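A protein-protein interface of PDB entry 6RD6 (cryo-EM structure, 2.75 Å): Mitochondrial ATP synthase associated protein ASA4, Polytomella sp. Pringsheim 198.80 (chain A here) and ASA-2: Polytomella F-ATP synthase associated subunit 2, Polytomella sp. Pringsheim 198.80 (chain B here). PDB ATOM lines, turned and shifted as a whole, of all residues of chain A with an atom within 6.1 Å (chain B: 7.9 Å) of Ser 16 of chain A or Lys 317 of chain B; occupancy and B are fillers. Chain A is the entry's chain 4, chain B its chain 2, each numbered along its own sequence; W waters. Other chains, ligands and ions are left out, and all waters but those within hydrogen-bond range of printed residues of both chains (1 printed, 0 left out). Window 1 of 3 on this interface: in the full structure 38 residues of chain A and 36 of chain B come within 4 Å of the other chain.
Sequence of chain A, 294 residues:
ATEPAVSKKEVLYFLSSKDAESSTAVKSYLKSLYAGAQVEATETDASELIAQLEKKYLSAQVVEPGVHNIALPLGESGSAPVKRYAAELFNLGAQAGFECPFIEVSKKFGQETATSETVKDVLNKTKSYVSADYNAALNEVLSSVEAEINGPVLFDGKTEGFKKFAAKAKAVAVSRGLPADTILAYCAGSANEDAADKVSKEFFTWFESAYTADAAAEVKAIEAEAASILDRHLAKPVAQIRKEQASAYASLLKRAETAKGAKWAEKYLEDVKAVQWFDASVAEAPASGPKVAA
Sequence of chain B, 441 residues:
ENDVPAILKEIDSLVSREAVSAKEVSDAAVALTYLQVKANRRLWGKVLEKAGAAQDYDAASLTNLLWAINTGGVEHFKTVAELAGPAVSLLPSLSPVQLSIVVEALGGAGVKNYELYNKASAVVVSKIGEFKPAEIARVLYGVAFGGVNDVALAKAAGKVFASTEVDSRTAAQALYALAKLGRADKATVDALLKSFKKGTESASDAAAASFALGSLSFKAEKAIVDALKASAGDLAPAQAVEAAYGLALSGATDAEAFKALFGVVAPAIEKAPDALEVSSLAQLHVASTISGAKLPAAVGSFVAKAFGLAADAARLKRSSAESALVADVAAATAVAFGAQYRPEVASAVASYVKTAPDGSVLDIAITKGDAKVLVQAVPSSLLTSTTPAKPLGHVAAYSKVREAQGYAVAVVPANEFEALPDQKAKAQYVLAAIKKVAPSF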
ATOM      1  N   VAL A  11     -30.351 -14.575  34.588  1.00  0.00           N
ATOM      2  CA  VAL A  11     -29.119 -15.068  33.977  1.00  0.00           C
ATOM      3  C   VAL A  11     -28.898 -14.411  32.617  1.00  0.00           C
ATOM      4  O   VAL A  11     -27.756 -14.158  32.217  1.00  0.00           O
ATOM      5  CB  VAL A  11     -29.123 -16.612  33.904  1.00  0.00           C
ATOM      6  CG1 VAL A  11     -30.150 -17.151  32.925  1.00  0.00           C
ATOM      7  CG2 VAL A  11     -27.741 -17.144  33.578  1.00  0.00           C
ATOM      8  N   LEU A  12     -29.984 -14.036  31.932  1.00  0.00           N
ATOM      9  CA  LEU A  12     -29.857 -13.328  30.663  1.00  0.00           C
ATOM     10  C   LEU A  12     -29.378 -11.903  30.885  1.00  0.00           C
ATOM     11  O   LEU A  12     -28.652 -11.343  30.056  1.00  0.00           O
ATOM     12  CB  LEU A  12     -31.189 -13.332  29.920  1.00  0.00           C
ATOM     13  CG  LEU A  12     -31.649 -14.667  29.349  1.00  0.00           C
ATOM     14  CD1 LEU A  12     -33.047 -14.534  28.789  1.00  0.00           C
ATOM     15  CD2 LEU A  12     -30.687 -15.166  28.306  1.00  0.00           C
ATOM     16  N   TYR A  13     -29.772 -11.296  32.005  1.00  0.00           N
ATOM     17  CA  TYR A  13     -29.214  -9.989  32.335  1.00  0.00           C
ATOM     18  C   TYR A  13     -27.791 -10.099  32.860  1.00  0.00           C
ATOM     19  O   TYR A  13     -27.026  -9.131  32.799  1.00  0.00           O
ATOM     20  CB  TYR A  13     -30.111  -9.267  33.333  1.00  0.00           C
ATOM     21  CG  TYR A  13     -31.030  -8.314  32.640  1.00  0.00           C
ATOM     22  CD1 TYR A  13     -30.703  -6.972  32.519  1.00  0.00           C
ATOM     23  CD2 TYR A  13     -32.192  -8.767  32.042  1.00  0.00           C
ATOM     24  CE1 TYR A  13     -31.533  -6.102  31.860  1.00  0.00           C
ATOM     25  CE2 TYR A  13     -33.027  -7.908  31.382  1.00  0.00           C
ATOM     26  CZ  TYR A  13     -32.692  -6.579  31.292  1.00  0.00           C
ATOM     27  OH  TYR A  13     -33.528  -5.728  30.626  1.00  0.00           O
ATOM     28  N   PHE A  14     -27.411 -11.266  33.368  1.00  0.00           N
ATOM     29  CA  PHE A  14     -26.077 -11.425  33.930  1.00  0.00           C
ATOM     30  C   PHE A  14     -25.077 -12.022  32.948  1.00  0.00           C
ATOM     31  O   PHE A  14     -23.922 -12.224  33.333  1.00  0.00           O
ATOM     32  CB  PHE A  14     -26.115 -12.300  35.188  1.00  0.00           C
ATOM     33  CG  PHE A  14     -26.904 -11.717  36.334  1.00  0.00           C
ATOM     34  CD1 PHE A  14     -27.165 -10.359  36.420  1.00  0.00           C
ATOM     35  CD2 PHE A  14     -27.391 -12.548  37.328  1.00  0.00           C
ATOM     36  CE1 PHE A  14     -27.901  -9.848  37.470  1.00  0.00           C
ATOM     37  CE2 PHE A  14     -28.124 -12.041  38.380  1.00  0.00           C
ATOM     38  CZ  PHE A  14     -28.376 -10.689  38.451  1.00  0.00           C
ATOM     39  N   LEU A  15     -25.491 -12.332  31.711  1.00  0.00           N
ATOM     40  CA  LEU A  15     -24.558 -12.876  30.723  1.00  0.00           C
ATOM     41  C   LEU A  15     -23.471 -11.873  30.357  1.00  0.00           C
ATOM     42  O   LEU A  15     -22.287 -12.222  30.316  1.00  0.00           O
ATOM     43  CB  LEU A  15     -25.300 -13.300  29.455  1.00  0.00           C
ATOM     44  CG  LEU A  15     -26.149 -14.567  29.436  1.00  0.00           C
ATOM     45  CD1 LEU A  15     -26.403 -15.011  28.013  1.00  0.00           C
ATOM     46  CD2 LEU A  15     -25.516 -15.674  30.256  1.00  0.00           C
ATOM     47  N   SER A  16     -23.849 -10.629  30.083  1.00  0.00           N
ATOM     48  CA  SER A  16     -22.887  -9.604  29.706  1.00  0.00           C
ATOM     49  C   SER A  16     -22.284  -8.884  30.901  1.00  0.00           C
ATOM     50  O   SER A  16     -21.494  -7.954  30.711  1.00  0.00           O
ATOM     51  CB  SER A  16     -23.540  -8.577  28.777  1.00  0.00           C
ATOM     52  OG  SER A  16     -22.631  -7.544  28.445  1.00  0.00           O
ATOM     53  N   SER A  17     -22.634  -9.284  32.119  1.00  0.00           N
ATOM     54  CA  SER A  17     -22.087  -8.645  33.304  1.00  0.00           C
ATOM     55  C   SER A  17     -20.655  -9.096  33.558  1.00  0.00           C
ATOM     56  O   SER A  17     -20.197 -10.112  33.030  1.00  0.00           O
ATOM     57  CB  SER A  17     -22.950  -8.960  34.522  1.00  0.00           C
ATOM     58  OG  SER A  17     -22.377  -8.424  35.698  1.00  0.00           O
ATOM     59  N   LYS A  18     -19.947  -8.320  34.373  1.00  0.00           N
ATOM     60  CA  LYS A  18     -18.597  -8.638  34.810  1.00  0.00           C
ATOM     61  C   LYS A  18     -18.507  -8.746  36.324  1.00  0.00           C
ATOM     62  O   LYS A  18     -17.410  -8.901  36.866  1.00  0.00           O
ATOM     63  CB  LYS A  18     -17.612  -7.588  34.294  1.00  0.00           C
ATOM     64  CG  LYS A  18     -17.573  -7.477  32.781  1.00  0.00           C
ATOM     65  CD  LYS A  18     -17.103  -8.771  32.144  1.00  0.00           C
ATOM     66  CE  LYS A  18     -16.870  -8.592  30.657  1.00  0.00           C
ATOM     67  NZ  LYS A  18     -18.022  -7.911  30.006  1.00  0.00           N
ATOM     68  N   LYS A  55     -37.504  -4.936  33.667  1.00  0.00           N
ATOM     69  CA  LYS A  55     -36.235  -4.453  33.135  1.00  0.00           C
ATOM     70  C   LYS A  55     -35.570  -3.474  34.091  1.00  0.00           C
ATOM     71  O   LYS A  55     -34.346  -3.505  34.267  1.00  0.00           O
ATOM     72  CB  LYS A  55     -36.471  -3.807  31.770  1.00  0.00           C
ATOM     73  CG  LYS A  55     -35.286  -3.067  31.177  1.00  0.00           C
ATOM     74  CD  LYS A  55     -35.456  -2.898  29.678  1.00  0.00           C
ATOM     75  CE  LYS A  55     -34.168  -2.443  29.017  1.00  0.00           C
ATOM     76  NZ  LYS A  55     -33.825  -1.042  29.378  1.00  0.00           N
ATOM     77  N   VAL A  62     -28.128  -5.468  38.269  1.00  0.00           N
ATOM     78  CA  VAL A  62     -26.793  -5.445  37.669  1.00  0.00           C
ATOM     79  C   VAL A  62     -25.991  -4.236  38.160  1.00  0.00           C
ATOM     80  O   VAL A  62     -24.790  -4.344  38.430  1.00  0.00           O
ATOM     81  CB  VAL A  62     -26.892  -5.485  36.133  1.00  0.00           C
ATOM     82  CG1 VAL A  62     -25.517  -5.497  35.501  1.00  0.00           C
ATOM     83  CG2 VAL A  62     -27.653  -6.705  35.690  1.00  0.00           C
ATOM     84  N   ALA A  94     -23.807   0.081  30.372  1.00  0.00           N
ATOM     85  CA  ALA A  94     -23.908  -0.761  29.186  1.00  0.00           C
ATOM     86  C   ALA A  94     -24.095  -2.227  29.558  1.00  0.00           C
ATOM     87  O   ALA A  94     -24.770  -2.974  28.841  1.00  0.00           O
ATOM     88  CB  ALA A  94     -22.670  -0.585  28.311  1.00  0.00           C
ATOM     89  N   GLN A  95     -23.510  -2.657  30.677  1.00  0.00           N
ATOM     90  CA  GLN A  95     -23.658  -4.044  31.105  1.00  0.00           C
ATOM     91  C   GLN A  95     -25.048  -4.309  31.666  1.00  0.00           C
ATOM     92  O   GLN A  95     -25.525  -5.448  31.648  1.00  0.00           O
ATOM     93  CB  GLN A  95     -22.595  -4.390  32.144  1.00  0.00           C
ATOM     94  CG  GLN A  95     -21.233  -4.699  31.565  1.00  0.00           C
ATOM     95  CD  GLN A  95     -20.110  -4.357  32.522  1.00  0.00           C
ATOM     96  OE1 GLN A  95     -20.284  -4.386  33.739  1.00  0.00           O
ATOM     97  NE2 GLN A  95     -18.949  -4.022  31.973  1.00  0.00           N
ATOM     98  N   ALA A  96     -25.709  -3.275  32.175  1.00  0.00           N
ATOM     99  CA  ALA A  96     -27.026  -3.431  32.773  1.00  0.00           C
ATOM    100  C   ALA A  96     -28.159  -3.237  31.781  1.00  0.00           C
ATOM    101  O   ALA A  96     -29.323  -3.347  32.170  1.00  0.00           O
ATOM    102  CB  ALA A  96     -27.194  -2.451  33.927  1.00  0.00           C
ATOM    103  N   GLY A  97     -27.857  -2.952  30.525  1.00  0.00           N
ATOM    104  CA  GLY A  97     -28.879  -2.815  29.519  1.00  0.00           C
ATOM    105  C   GLY A  97     -29.296  -1.401  29.207  1.00  0.00           C
ATOM    106  O   GLY A  97     -30.300  -1.214  28.513  1.00  0.00           O
ATOM    107  N   GLU B 277     -17.000 -17.092  27.105  1.00  0.00           N
ATOM    108  CA  GLU B 277     -18.202 -16.284  27.210  1.00  0.00           C
ATOM    109  C   GLU B 277     -19.317 -16.893  26.372  1.00  0.00           C
ATOM    110  O   GLU B 277     -19.070 -17.680  25.456  1.00  0.00           O
ATOM    111  CB  GLU B 277     -17.927 -14.852  26.757  1.00  0.00           C
ATOM    112  CG  GLU B 277     -17.147 -14.031  27.762  1.00  0.00           C
ATOM    113  CD  GLU B 277     -18.045 -13.222  28.673  1.00  0.00           C
ATOM    114  OE1 GLU B 277     -18.813 -12.382  28.160  1.00  0.00           O
ATOM    115  OE2 GLU B 277     -17.985 -13.427  29.903  1.00  0.00           O
ATOM    116  N   VAL B 278     -20.556 -16.517  26.693  1.00  0.00           N
ATOM    117  CA  VAL B 278     -21.713 -17.075  25.996  1.00  0.00           C
ATOM    118  C   VAL B 278     -21.795 -16.529  24.575  1.00  0.00           C
ATOM    119  O   VAL B 278     -22.308 -17.194  23.666  1.00  0.00           O
ATOM    120  CB  VAL B 278     -22.993 -16.795  26.803  1.00  0.00           C
ATOM    121  CG1 VAL B 278     -24.154 -17.630  26.302  1.00  0.00           C
ATOM    122  CG2 VAL B 278     -22.739 -17.097  28.257  1.00  0.00           C
ATOM    123  N   SER B 279     -21.263 -15.326  24.354  1.00  0.00           N
ATOM    124  CA  SER B 279     -21.155 -14.803  22.996  1.00  0.00           C
ATOM    125  C   SER B 279     -20.177 -15.619  22.163  1.00  0.00           C
ATOM    126  O   SER B 279     -20.413 -15.839  20.971  1.00  0.00           O
ATOM    127  CB  SER B 279     -20.733 -13.337  23.029  1.00  0.00           C
ATOM    128  OG  SER B 279     -19.508 -13.178  23.717  1.00  0.00           O
ATOM    129  N   ALA B 311     -28.927 -14.974  21.939  1.00  0.00           N
ATOM    130  CA  ALA B 311     -29.978 -14.275  21.203  1.00  0.00           C
ATOM    131  C   ALA B 311     -31.019 -13.685  22.147  1.00  0.00           C
ATOM    132  O   ALA B 311     -31.464 -12.545  21.954  1.00  0.00           O
ATOM    133  CB  ALA B 311     -30.635 -15.224  20.204  1.00  0.00           C
ATOM    134  N   ASP B 312     -31.389 -14.431  23.195  1.00  0.00           N
ATOM    135  CA  ASP B 312     -32.324 -13.910  24.189  1.00  0.00           C
ATOM    136  C   ASP B 312     -31.735 -12.734  24.958  1.00  0.00           C
ATOM    137  O   ASP B 312     -32.444 -11.780  25.293  1.00  0.00           O
ATOM    138  CB  ASP B 312     -32.718 -15.017  25.158  1.00  0.00           C
ATOM    139  CG  ASP B 312     -33.985 -15.708  24.758  1.00  0.00           C
ATOM    140  OD1 ASP B 312     -34.748 -15.131  23.957  1.00  0.00           O
ATOM    141  OD2 ASP B 312     -34.227 -16.823  25.262  1.00  0.00           O
ATOM    142  N   ALA B 313     -30.435 -12.788  25.251  1.00  0.00           N
ATOM    143  CA  ALA B 313     -29.800 -11.708  25.995  1.00  0.00           C
ATOM    144  C   ALA B 313     -29.637 -10.466  25.135  1.00  0.00           C
ATOM    145  O   ALA B 313     -29.701  -9.341  25.640  1.00  0.00           O
ATOM    146  CB  ALA B 313     -28.449 -12.170  26.535  1.00  0.00           C
ATOM    147  N   ALA B 314     -29.426 -10.647  23.830  1.00  0.00           N
ATOM    148  CA  ALA B 314     -29.394  -9.499  22.934  1.00  0.00           C
ATOM    149  C   ALA B 314     -30.786  -8.933  22.698  1.00  0.00           C
ATOM    150  O   ALA B 314     -30.921  -7.763  22.330  1.00  0.00           O
ATOM    151  CB  ALA B 314     -28.743  -9.884  21.608  1.00  0.00           C
ATOM    152  N   ARG B 315     -31.828  -9.744  22.887  1.00  0.00           N
ATOM    153  CA  ARG B 315     -33.185  -9.221  22.756  1.00  0.00           C
ATOM    154  C   ARG B 315     -33.651  -8.507  24.023  1.00  0.00           C
ATOM    155  O   ARG B 315     -34.418  -7.543  23.942  1.00  0.00           O
ATOM    156  CB  ARG B 315     -34.151 -10.349  22.400  1.00  0.00           C
ATOM    157  CG  ARG B 315     -35.497  -9.863  21.907  1.00  0.00           C
ATOM    158  CD  ARG B 315     -36.530 -10.959  21.935  1.00  0.00           C
ATOM    159  NE  ARG B 315     -37.852 -10.449  21.598  1.00  0.00           N
ATOM    160  CZ  ARG B 315     -38.755 -10.073  22.495  1.00  0.00           C
ATOM    161  NH1 ARG B 315     -38.479 -10.154  23.788  1.00  0.00           N
ATOM    162  NH2 ARG B 315     -39.935  -9.620  22.101  1.00  0.00           N
ATOM    163  N   LEU B 316     -33.221  -8.972  25.198  1.00  0.00           N
ATOM    164  CA  LEU B 316     -33.639  -8.333  26.445  1.00  0.00           C
ATOM    165  C   LEU B 316     -32.992  -6.968  26.621  1.00  0.00           C
ATOM    166  O   LEU B 316     -33.667  -5.998  26.983  1.00  0.00           O
ATOM    167  CB  LEU B 316     -33.307  -9.221  27.638  1.00  0.00           C
ATOM    168  CG  LEU B 316     -34.435 -10.084  28.180  1.00  0.00           C
ATOM    169  CD1 LEU B 316     -33.933 -10.886  29.348  1.00  0.00           C
ATOM    170  CD2 LEU B 316     -35.593  -9.210  28.602  1.00  0.00           C
ATOM    171  N   LYS B 317     -31.690  -6.871  26.370  1.00  0.00           N
ATOM    172  CA  LYS B 317     -30.954  -5.624  26.495  1.00  0.00           C
ATOM    173  C   LYS B 317     -30.881  -4.878  25.171  1.00  0.00           C
ATOM    174  O   LYS B 317     -29.884  -4.207  24.890  1.00  0.00           O
ATOM    175  CB  LYS B 317     -29.562  -5.903  27.059  1.00  0.00           C
ATOM    176  CG  LYS B 317     -29.599  -6.923  28.189  1.00  0.00           C
ATOM    177  CD  LYS B 317     -28.631  -6.599  29.305  1.00  0.00           C
ATOM    178  CE  LYS B 317     -27.210  -6.932  28.914  1.00  0.00           C
ATOM    179  NZ  LYS B 317     -26.354  -7.126  30.109  1.00  0.00           N
ATOM    180  N   ARG B 318     -31.923  -5.007  24.358  1.00  0.00           N
ATOM    181  CA  ARG B 318     -32.022  -4.353  23.064  1.00  0.00           C
ATOM    182  C   ARG B 318     -32.148  -2.842  23.227  1.00  0.00           C
ATOM    183  O   ARG B 318     -32.727  -2.348  24.198  1.00  0.00           O
ATOM    184  CB  ARG B 318     -33.236  -4.919  22.322  1.00  0.00           C
ATOM    185  CG  ARG B 318     -33.468  -4.396  20.938  1.00  0.00           C
ATOM    186  CD  ARG B 318     -34.845  -4.723  20.431  1.00  0.00           C
ATOM    187  NE  ARG B 318     -34.875  -6.015  19.766  1.00  0.00           N
ATOM    188  CZ  ARG B 318     -35.930  -6.815  19.743  1.00  0.00           C
ATOM    189  NH1 ARG B 318     -37.056  -6.451  20.340  1.00  0.00           N
ATOM    190  NH2 ARG B 318     -35.856  -7.970  19.109  1.00  0.00           N
ATOM    191  N   SER B 319     -31.577  -2.107  22.273  1.00  0.00           N
ATOM    192  CA  SER B 319     -31.782  -0.669  22.176  1.00  0.00           C
ATOM    193  C   SER B 319     -33.251  -0.338  21.925  1.00  0.00           C
ATOM    194  O   SER B 319     -34.013  -1.146  21.394  1.00  0.00           O
ATOM    195  CB  SER B 319     -30.923  -0.091  21.056  1.00  0.00           C
ATOM    196  OG  SER B 319     -31.168   1.293  20.896  1.00  0.00           O
ATOM    197  N   SER B 320     -33.648   0.873  22.318  1.00  0.00           N
ATOM    198  CA  SER B 320     -35.049   1.263  22.192  1.00  0.00           C
ATOM    199  C   SER B 320     -35.398   1.624  20.755  1.00  0.00           C
ATOM    200  O   SER B 320     -36.549   1.466  20.330  1.00  0.00           O
ATOM    201  CB  SER B 320     -35.354   2.431  23.119  1.00  0.00           C
ATOM    202  OG  SER B 320     -34.395   3.460  22.956  1.00  0.00           O
ATOM    203  N   GLU B 322     -34.113   0.026  18.225  1.00  0.00           N
ATOM    204  CA  GLU B 322     -34.316  -1.277  17.605  1.00  0.00           C
ATOM    205  C   GLU B 322     -35.662  -1.870  18.002  1.00  0.00           C
ATOM    206  O   GLU B 322     -36.294  -2.567  17.203  1.00  0.00           O
ATOM    207  CB  GLU B 322     -33.176  -2.222  17.971  1.00  0.00           C
ATOM    208  CG  GLU B 322     -33.192  -3.523  17.192  1.00  0.00           C
ATOM    209  CD  GLU B 322     -32.180  -4.525  17.692  1.00  0.00           C
ATOM    210  OE1 GLU B 322     -31.124  -4.099  18.207  1.00  0.00           O
ATOM    211  OE2 GLU B 322     -32.443  -5.739  17.578  1.00  0.00           O
ATOM    212  N   SER B 323     -36.135  -1.577  19.217  1.00  0.00           N
ATOM    213  CA  SER B 323     -37.472  -2.013  19.616  1.00  0.00           C
ATOM    214  C   SER B 323     -38.547  -1.303  18.805  1.00  0.00           C
ATOM    215  O   SER B 323     -39.532  -1.925  18.385  1.00  0.00           O
ATOM    216  CB  SER B 323     -37.690  -1.765  21.106  1.00  0.00           C
ATOM    217  OG  SER B 323     -36.833  -2.563  21.896  1.00  0.00           O
HETATM  218  O   HOH W   1     -26.504 -10.222  28.620  1.00  0.00           O
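NZ of Lys 317 of chain B sits at hydrogen-bond distance from O of Tyr 13 of chain A (3.4 Å). NZ of Lys 317 of chain B sits at hydrogen-bond distance from O of Gln 95 of chain A.
Among the printed residues, merely in contact across the chains: Ser 16 of chain A with Lys 317 of chain B (3.4 Å), Leu 12 of chain A with Ala 313 of chain B (3.6 Å), Tyr 13 of chain A with Leu 316 of chain B (3.7 Å), Leu 12 of chain A with Asp 312 of chain B (3.7 Å), Leu 15 of chain A with Val 278 of chain B (3.7 Å), Leu 12 of chain A with Leu 316 of chain B (3.7 Å), Gly 97 of chain A with Lys 317 of chain B (3.8 Å) and Leu 15 of chain A with Ala 313 of chain B (3.8 Å).
Ser 16 of chain A touches one residue of chain B. Lys 55 of chain A touches none of the printed residues of chain B. Of the printed residues of chain B, Gln 95 of chain A touches Lys 317. Of the printed residues of chain B, Gly 97 of chain A touches Lys 317 (3.8 Å). Lys 317 of chain B touches just these residues of chain A: Tyr 13 (3.4 Å), Ser 16 (3.4 Å), Gln 95 (2.4 Å) and Gly 97 (3.8 Å). Glu 322 of chain B touches none of the printed residues of chain A. The nearest residue of chain B that does not touch Ser 16 of chain A is Glu 277 of chain B (5.2 Å). The nearest printed residue of chain B that does not touch Gln 95 of chain A is Ala 313 of chain B (8.3 Å).
Of the 14 printed residues of chain A, 6 touch a printed residue of chain B. Hydrophobic or aromatic side chains of chain A that line the printed part of chain B: Leu 12, Tyr 13 and Leu 15. Hydrophobic or aromatic side chains of chain B that line the printed part of chain A: Val 278, Ala 313 and Leu 316. Among the printed residues, no Asp or Glu carboxylate lies within 4 Å of a Lys or Arg side-chain nitrogen of the other chain.
Water W1 lies within hydrogen-bond range of O of Leu 12 of chain A (2.8 Å), N of Ser 16 of chain A (3.1 Å) and NZ of Lys 317 of chain B (3.4 Å).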
